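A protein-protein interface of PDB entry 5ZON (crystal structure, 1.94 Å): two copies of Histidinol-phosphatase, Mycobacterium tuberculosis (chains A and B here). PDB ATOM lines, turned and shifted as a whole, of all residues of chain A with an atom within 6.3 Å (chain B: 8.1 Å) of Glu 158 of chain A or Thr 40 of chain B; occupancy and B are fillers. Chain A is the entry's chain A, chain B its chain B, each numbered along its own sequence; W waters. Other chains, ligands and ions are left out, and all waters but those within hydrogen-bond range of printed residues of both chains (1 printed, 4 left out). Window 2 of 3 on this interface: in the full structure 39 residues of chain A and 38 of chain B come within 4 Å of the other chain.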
ATOM      1  N   SER A 155     -16.475 -11.808  18.107  1.00  0.00           N
ATOM      2  CA  SER A 155     -16.920 -11.346  16.775  1.00  0.00           C
ATOM      3  C   SER A 155     -15.844 -10.497  16.081  1.00  0.00           C
ATOM      4  O   SER A 155     -16.151  -9.745  15.170  1.00  0.00           O
ATOM      5  CB  SER A 155     -18.219 -10.583  16.880  1.00  0.00           C
ATOM      6  OG  SER A 155     -19.221 -11.419  17.408  1.00  0.00           O
ATOM      7  N   VAL A 156     -14.587 -10.644  16.493  1.00  0.00           N
ATOM      8  CA  VAL A 156     -13.507  -9.840  15.941  1.00  0.00           C
ATOM      9  C   VAL A 156     -13.303 -10.243  14.479  1.00  0.00           C
ATOM     10  O   VAL A 156     -13.096 -11.419  14.163  1.00  0.00           O
ATOM     11  CB  VAL A 156     -12.230 -10.052  16.784  1.00  0.00           C
ATOM     12  CG1 VAL A 156     -11.034  -9.403  16.116  1.00  0.00           C
ATOM     13  CG2 VAL A 156     -12.399  -9.509  18.201  1.00  0.00           C
ATOM     14  N   ALA A 157     -13.370  -9.287  13.571  1.00  0.00           N
ATOM     15  CA  ALA A 157     -13.390  -9.647  12.145  1.00  0.00           C
ATOM     16  C   ALA A 157     -12.108  -9.162  11.457  1.00  0.00           C
ATOM     17  O   ALA A 157     -11.800  -9.562  10.352  1.00  0.00           O
ATOM     18  CB  ALA A 157     -14.640  -9.130  11.464  1.00  0.00           C
ATOM     19  N   GLU A 158     -11.334  -8.347  12.123  1.00  0.00           N
ATOM     20  CA  GLU A 158     -10.107  -7.859  11.514  1.00  0.00           C
ATOM     21  C   GLU A 158      -8.912  -8.465  12.261  1.00  0.00           C
ATOM     22  O   GLU A 158      -8.806  -8.356  13.480  1.00  0.00           O
ATOM     23  CB  GLU A 158     -10.018  -6.327  11.501  1.00  0.00           C
ATOM     24  CG  GLU A 158     -11.276  -5.536  11.866  1.00  0.00           C
ATOM     25  CD  GLU A 158     -11.067  -4.060  12.221  1.00  0.00           C
ATOM     26  OE1 GLU A 158     -11.920  -3.478  12.954  1.00  0.00           O
ATOM     27  OE2 GLU A 158     -10.043  -3.487  11.769  1.00  0.00           O
ATOM     28  N   LEU A 159      -7.998  -9.044  11.494  1.00  0.00           N
ATOM     29  CA  LEU A 159      -6.776  -9.607  12.014  1.00  0.00           C
ATOM     30  C   LEU A 159      -6.037  -8.580  12.880  1.00  0.00           C
ATOM     31  O   LEU A 159      -5.484  -8.948  13.935  1.00  0.00           O
ATOM     32  CB  LEU A 159      -5.928 -10.036  10.820  1.00  0.00           C
ATOM     33  CG  LEU A 159      -4.938 -11.143  11.121  1.00  0.00           C
ATOM     34  CD1 LEU A 159      -5.666 -12.384  11.594  1.00  0.00           C
ATOM     35  CD2 LEU A 159      -4.140 -11.467   9.885  1.00  0.00           C
ATOM     36  N   HIS A 160      -6.003  -7.319  12.444  1.00  0.00           N
ATOM     37  CA  HIS A 160      -5.281  -6.255  13.161  1.00  0.00           C
ATOM     38  C   HIS A 160      -5.927  -5.953  14.524  1.00  0.00           C
ATOM     39  O   HIS A 160      -5.331  -5.273  15.351  1.00  0.00           O
ATOM     40  CB  HIS A 160      -5.144  -5.020  12.251  1.00  0.00           C
ATOM     41  CG  HIS A 160      -4.201  -5.258  11.117  1.00  0.00           C
ATOM     42  N   SER A 161      -7.134  -6.452  14.788  1.00  0.00           N
ATOM     43  CA  SER A 161      -7.740  -6.261  16.114  1.00  0.00           C
ATOM     44  C   SER A 161      -7.667  -7.542  16.972  1.00  0.00           C
ATOM     45  O   SER A 161      -8.165  -7.556  18.135  1.00  0.00           O
ATOM     46  CB  SER A 161      -9.174  -5.817  15.966  1.00  0.00           C
ATOM     47  OG  SER A 161      -9.177  -4.517  15.405  1.00  0.00           O
ATOM     48  N   ALA A 162      -7.101  -8.603  16.403  1.00  0.00           N
ATOM     49  CA  ALA A 162      -7.257  -9.933  16.986  1.00  0.00           C
ATOM     50  C   ALA A 162      -6.218 -10.174  18.077  1.00  0.00           C
ATOM     51  O   ALA A 162      -5.086  -9.652  18.027  1.00  0.00           O
ATOM     52  CB  ALA A 162      -7.116 -10.982  15.911  1.00  0.00           C
ATOM     53  N   LEU A 256     -12.079 -15.216  11.431  1.00  0.00           N
ATOM     54  CA  LEU A 256     -10.671 -14.904  11.082  1.00  0.00           C
ATOM     55  C   LEU A 256     -10.039 -16.111  10.368  1.00  0.00           C
ATOM     56  O   LEU A 256      -8.882 -16.056   9.893  1.00  0.00           O
ATOM     57  CB  LEU A 256      -9.908 -14.539  12.366  1.00  0.00           C
ATOM     58  CG  LEU A 256     -10.349 -13.249  13.064  1.00  0.00           C
ATOM     59  CD1 LEU A 256      -9.719 -13.126  14.444  1.00  0.00           C
ATOM     60  CD2 LEU A 256      -9.991 -12.013  12.238  1.00  0.00           C
ATOM     61  N   GLU A 259      -8.493 -15.950   6.728  1.00  0.00           N
ATOM     62  CA  GLU A 259      -7.336 -15.039   6.660  1.00  0.00           C
ATOM     63  C   GLU A 259      -6.118 -15.613   7.392  1.00  0.00           C
ATOM     64  O   GLU A 259      -4.991 -15.432   6.948  1.00  0.00           O
ATOM     65  CB  GLU A 259      -7.621 -13.635   7.207  1.00  0.00           C
ATOM     66  CG  GLU A 259      -6.487 -12.699   6.775  1.00  0.00           C
ATOM     67  CD  GLU A 259      -6.625 -11.214   7.029  1.00  0.00           C
ATOM     68  OE1 GLU A 259      -7.743 -10.794   7.426  1.00  0.00           O
ATOM     69  OE2 GLU A 259      -5.616 -10.493   6.846  1.00  0.00           O
ATOM     70  N   ARG B  37     -18.643  -9.721  24.648  1.00  0.00           N
ATOM     71  CA  ARG B  37     -18.893  -9.638  23.204  1.00  0.00           C
ATOM     72  C   ARG B  37     -18.112  -8.451  22.625  1.00  0.00           C
ATOM     73  O   ARG B  37     -18.088  -7.386  23.193  1.00  0.00           O
ATOM     74  CB  ARG B  37     -20.396  -9.593  22.919  1.00  0.00           C
ATOM     75  CG  ARG B  37     -21.100 -10.919  23.211  1.00  0.00           C
ATOM     76  CD  ARG B  37     -22.605 -11.005  22.963  1.00  0.00           C
ATOM     77  NE  ARG B  37     -23.377 -10.092  23.804  1.00  0.00           N
ATOM     78  CZ  ARG B  37     -24.410  -9.345  23.411  1.00  0.00           C
ATOM     79  NH1 ARG B  37     -25.282  -9.804  22.526  1.00  0.00           N
ATOM     80  NH2 ARG B  37     -24.557  -8.126  23.905  1.00  0.00           N
ATOM     81  N   ILE B  38     -17.436  -8.638  21.509  1.00  0.00           N
ATOM     82  CA  ILE B  38     -16.470  -7.643  21.035  1.00  0.00           C
ATOM     83  C   ILE B  38     -16.266  -7.862  19.530  1.00  0.00           C
ATOM     84  O   ILE B  38     -16.303  -9.005  19.070  1.00  0.00           O
ATOM     85  CB  ILE B  38     -15.140  -7.759  21.822  1.00  0.00           C
ATOM     86  CG1 ILE B  38     -14.101  -6.721  21.394  1.00  0.00           C
ATOM     87  CG2 ILE B  38     -14.563  -9.163  21.718  1.00  0.00           C
ATOM     88  CD1 ILE B  38     -13.068  -6.380  22.449  1.00  0.00           C
ATOM     89  N   ASP B  39     -16.020  -6.811  18.764  1.00  0.00           N
ATOM     90  CA  ASP B  39     -15.817  -7.026  17.320  1.00  0.00           C
ATOM     91  C   ASP B  39     -14.661  -6.174  16.798  1.00  0.00           C
ATOM     92  O   ASP B  39     -14.385  -6.180  15.608  1.00  0.00           O
ATOM     93  CB  ASP B  39     -17.130  -6.906  16.535  1.00  0.00           C
ATOM     94  CG  ASP B  39     -17.774  -5.525  16.547  1.00  0.00           C
ATOM     95  OD1 ASP B  39     -17.179  -4.597  17.122  1.00  0.00           O
ATOM     96  OD2 ASP B  39     -18.883  -5.391  15.977  1.00  0.00           O
ATOM     97  N   THR B  40     -13.980  -5.477  17.705  1.00  0.00           N
ATOM     98  CA  THR B  40     -12.828  -4.636  17.372  1.00  0.00           C
ATOM     99  C   THR B  40     -11.840  -4.630  18.550  1.00  0.00           C
ATOM    100  O   THR B  40     -12.003  -5.368  19.495  1.00  0.00           O
ATOM    101  CB  THR B  40     -13.299  -3.199  17.074  1.00  0.00           C
ATOM    102  OG1 THR B  40     -14.049  -2.777  18.213  1.00  0.00           O
ATOM    103  CG2 THR B  40     -14.246  -3.091  15.904  1.00  0.00           C
ATOM    104  N   LYS B  41     -10.819  -3.778  18.489  1.00  0.00           N
ATOM    105  CA  LYS B  41      -9.997  -3.449  19.649  1.00  0.00           C
ATOM    106  C   LYS B  41     -10.877  -3.067  20.847  1.00  0.00           C
ATOM    107  O   LYS B  41     -11.921  -2.431  20.660  1.00  0.00           O
ATOM    108  CB  LYS B  41      -9.009  -2.341  19.303  1.00  0.00           C
ATOM    109  CG  LYS B  41      -7.807  -2.836  18.505  1.00  0.00           C
ATOM    110  CD  LYS B  41      -6.722  -1.821  18.379  1.00  0.00           C
ATOM    111  CE  LYS B  41      -6.061  -1.883  17.022  1.00  0.00           C
ATOM    112  NZ  LYS B  41      -4.687  -1.329  17.066  1.00  0.00           N
ATOM    113  N   PRO B  42     -10.484  -3.485  22.075  1.00  0.00           N
ATOM    114  CA  PRO B  42     -11.448  -3.314  23.174  1.00  0.00           C
ATOM    115  C   PRO B  42     -11.372  -1.883  23.728  1.00  0.00           C
ATOM    116  O   PRO B  42     -10.303  -1.244  23.772  1.00  0.00           O
ATOM    117  CB  PRO B  42     -10.963  -4.266  24.278  1.00  0.00           C
ATOM    118  CG  PRO B  42      -9.446  -4.298  24.046  1.00  0.00           C
ATOM    119  CD  PRO B  42      -9.283  -4.204  22.541  1.00  0.00           C
ATOM    120  N   ASP B  43     -12.513  -1.415  24.194  1.00  0.00           N
ATOM    121  CA  ASP B  43     -12.611  -0.117  24.843  1.00  0.00           C
ATOM    122  C   ASP B  43     -12.163  -0.269  26.309  1.00  0.00           C
ATOM    123  O   ASP B  43     -12.721  -1.080  27.050  1.00  0.00           O
ATOM    124  CB  ASP B  43     -14.032   0.402  24.590  1.00  0.00           C
ATOM    125  CG  ASP B  43     -14.525   1.467  25.544  1.00  0.00           C
ATOM    126  OD1 ASP B  43     -13.777   2.447  25.751  1.00  0.00           O
ATOM    127  OD2 ASP B  43     -15.643   1.287  26.085  1.00  0.00           O
ATOM    128  N   ARG B 100     -10.745  -8.356  28.026  1.00  0.00           N
ATOM    129  CA  ARG B 100     -11.100  -9.412  27.070  1.00  0.00           C
ATOM    130  C   ARG B 100     -11.678 -10.601  27.835  1.00  0.00           C
ATOM    131  O   ARG B 100     -12.224 -11.507  27.206  1.00  0.00           O
ATOM    132  CB  ARG B 100      -9.919  -9.847  26.196  1.00  0.00           C
ATOM    133  CG  ARG B 100      -9.518  -8.818  25.141  1.00  0.00           C
ATOM    134  CD  ARG B 100     -10.532  -8.502  24.037  1.00  0.00           C
ATOM    135  NE  ARG B 100     -11.184  -9.706  23.511  1.00  0.00           N
ATOM    136  CZ  ARG B 100     -10.841 -10.332  22.388  1.00  0.00           C
ATOM    137  NH1 ARG B 100      -9.950  -9.804  21.554  1.00  0.00           N
ATOM    138  NH2 ARG B 100     -11.389 -11.500  22.105  1.00  0.00           N
HETATM  139  O   HOH W   1      -9.693  -7.122  20.671  1.00  0.00           O
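O of Ile 38 of chain B lies within hydrogen-bond range of N of Ser 155 of chain A, 3.0 Å away.
Asp 39 of chain B touches Ser 155 of chain A. N of Val 156 of chain A touches O of Ile 38 of chain B (3.5 Å). Val 156 of chain A touches Asp 39 of chain B. Ala 157 of chain A touches Asp 39 of chain B. Glu 158 of chain A touches Thr 40 of chain B (OE1 to CG2, 3.8 Å). Lys 41 of chain B touches His 160 of chain A. CB of Ser 161 of chain A touches C of Thr 40 of chain B (3.9 Å). N of Lys 41 of chain B touches OG of Ser 161 of chain A (3.6 Å).
Thr 40 of chain B touches two residues of chain A. Of chain B, only Asp 39 comes within 4 Å of Ala 157 of chain A. Of the printed residues of chain B, Val 156 of chain A touches Ile 38 (3.5 Å) and Asp 39 (3.8 Å). Printed residues of chain B within 4 Å of Ser 155 of chain A: Ile 38 and Asp 39. The nearest residue of chain B that does not touch Glu 158 of chain A is Asp 39 of chain B (4.5 Å).
Printed residues of chain A that touch a printed residue of chain B: Ser 155, Val 156, Ala 157, Glu 158, His 160 and Ser 161. Among the printed residues, 9 pairs touch across the chains.
No position is printed for both chains.
Water W1 lies within hydrogen-bond range of the guanidinium group (NH1) of Arg 100 of chain B, the backbone carbonyl oxygen (O) of Ser 161 of chain A and the backbone carbonyl oxygen (O) of Thr 40 of chain B.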
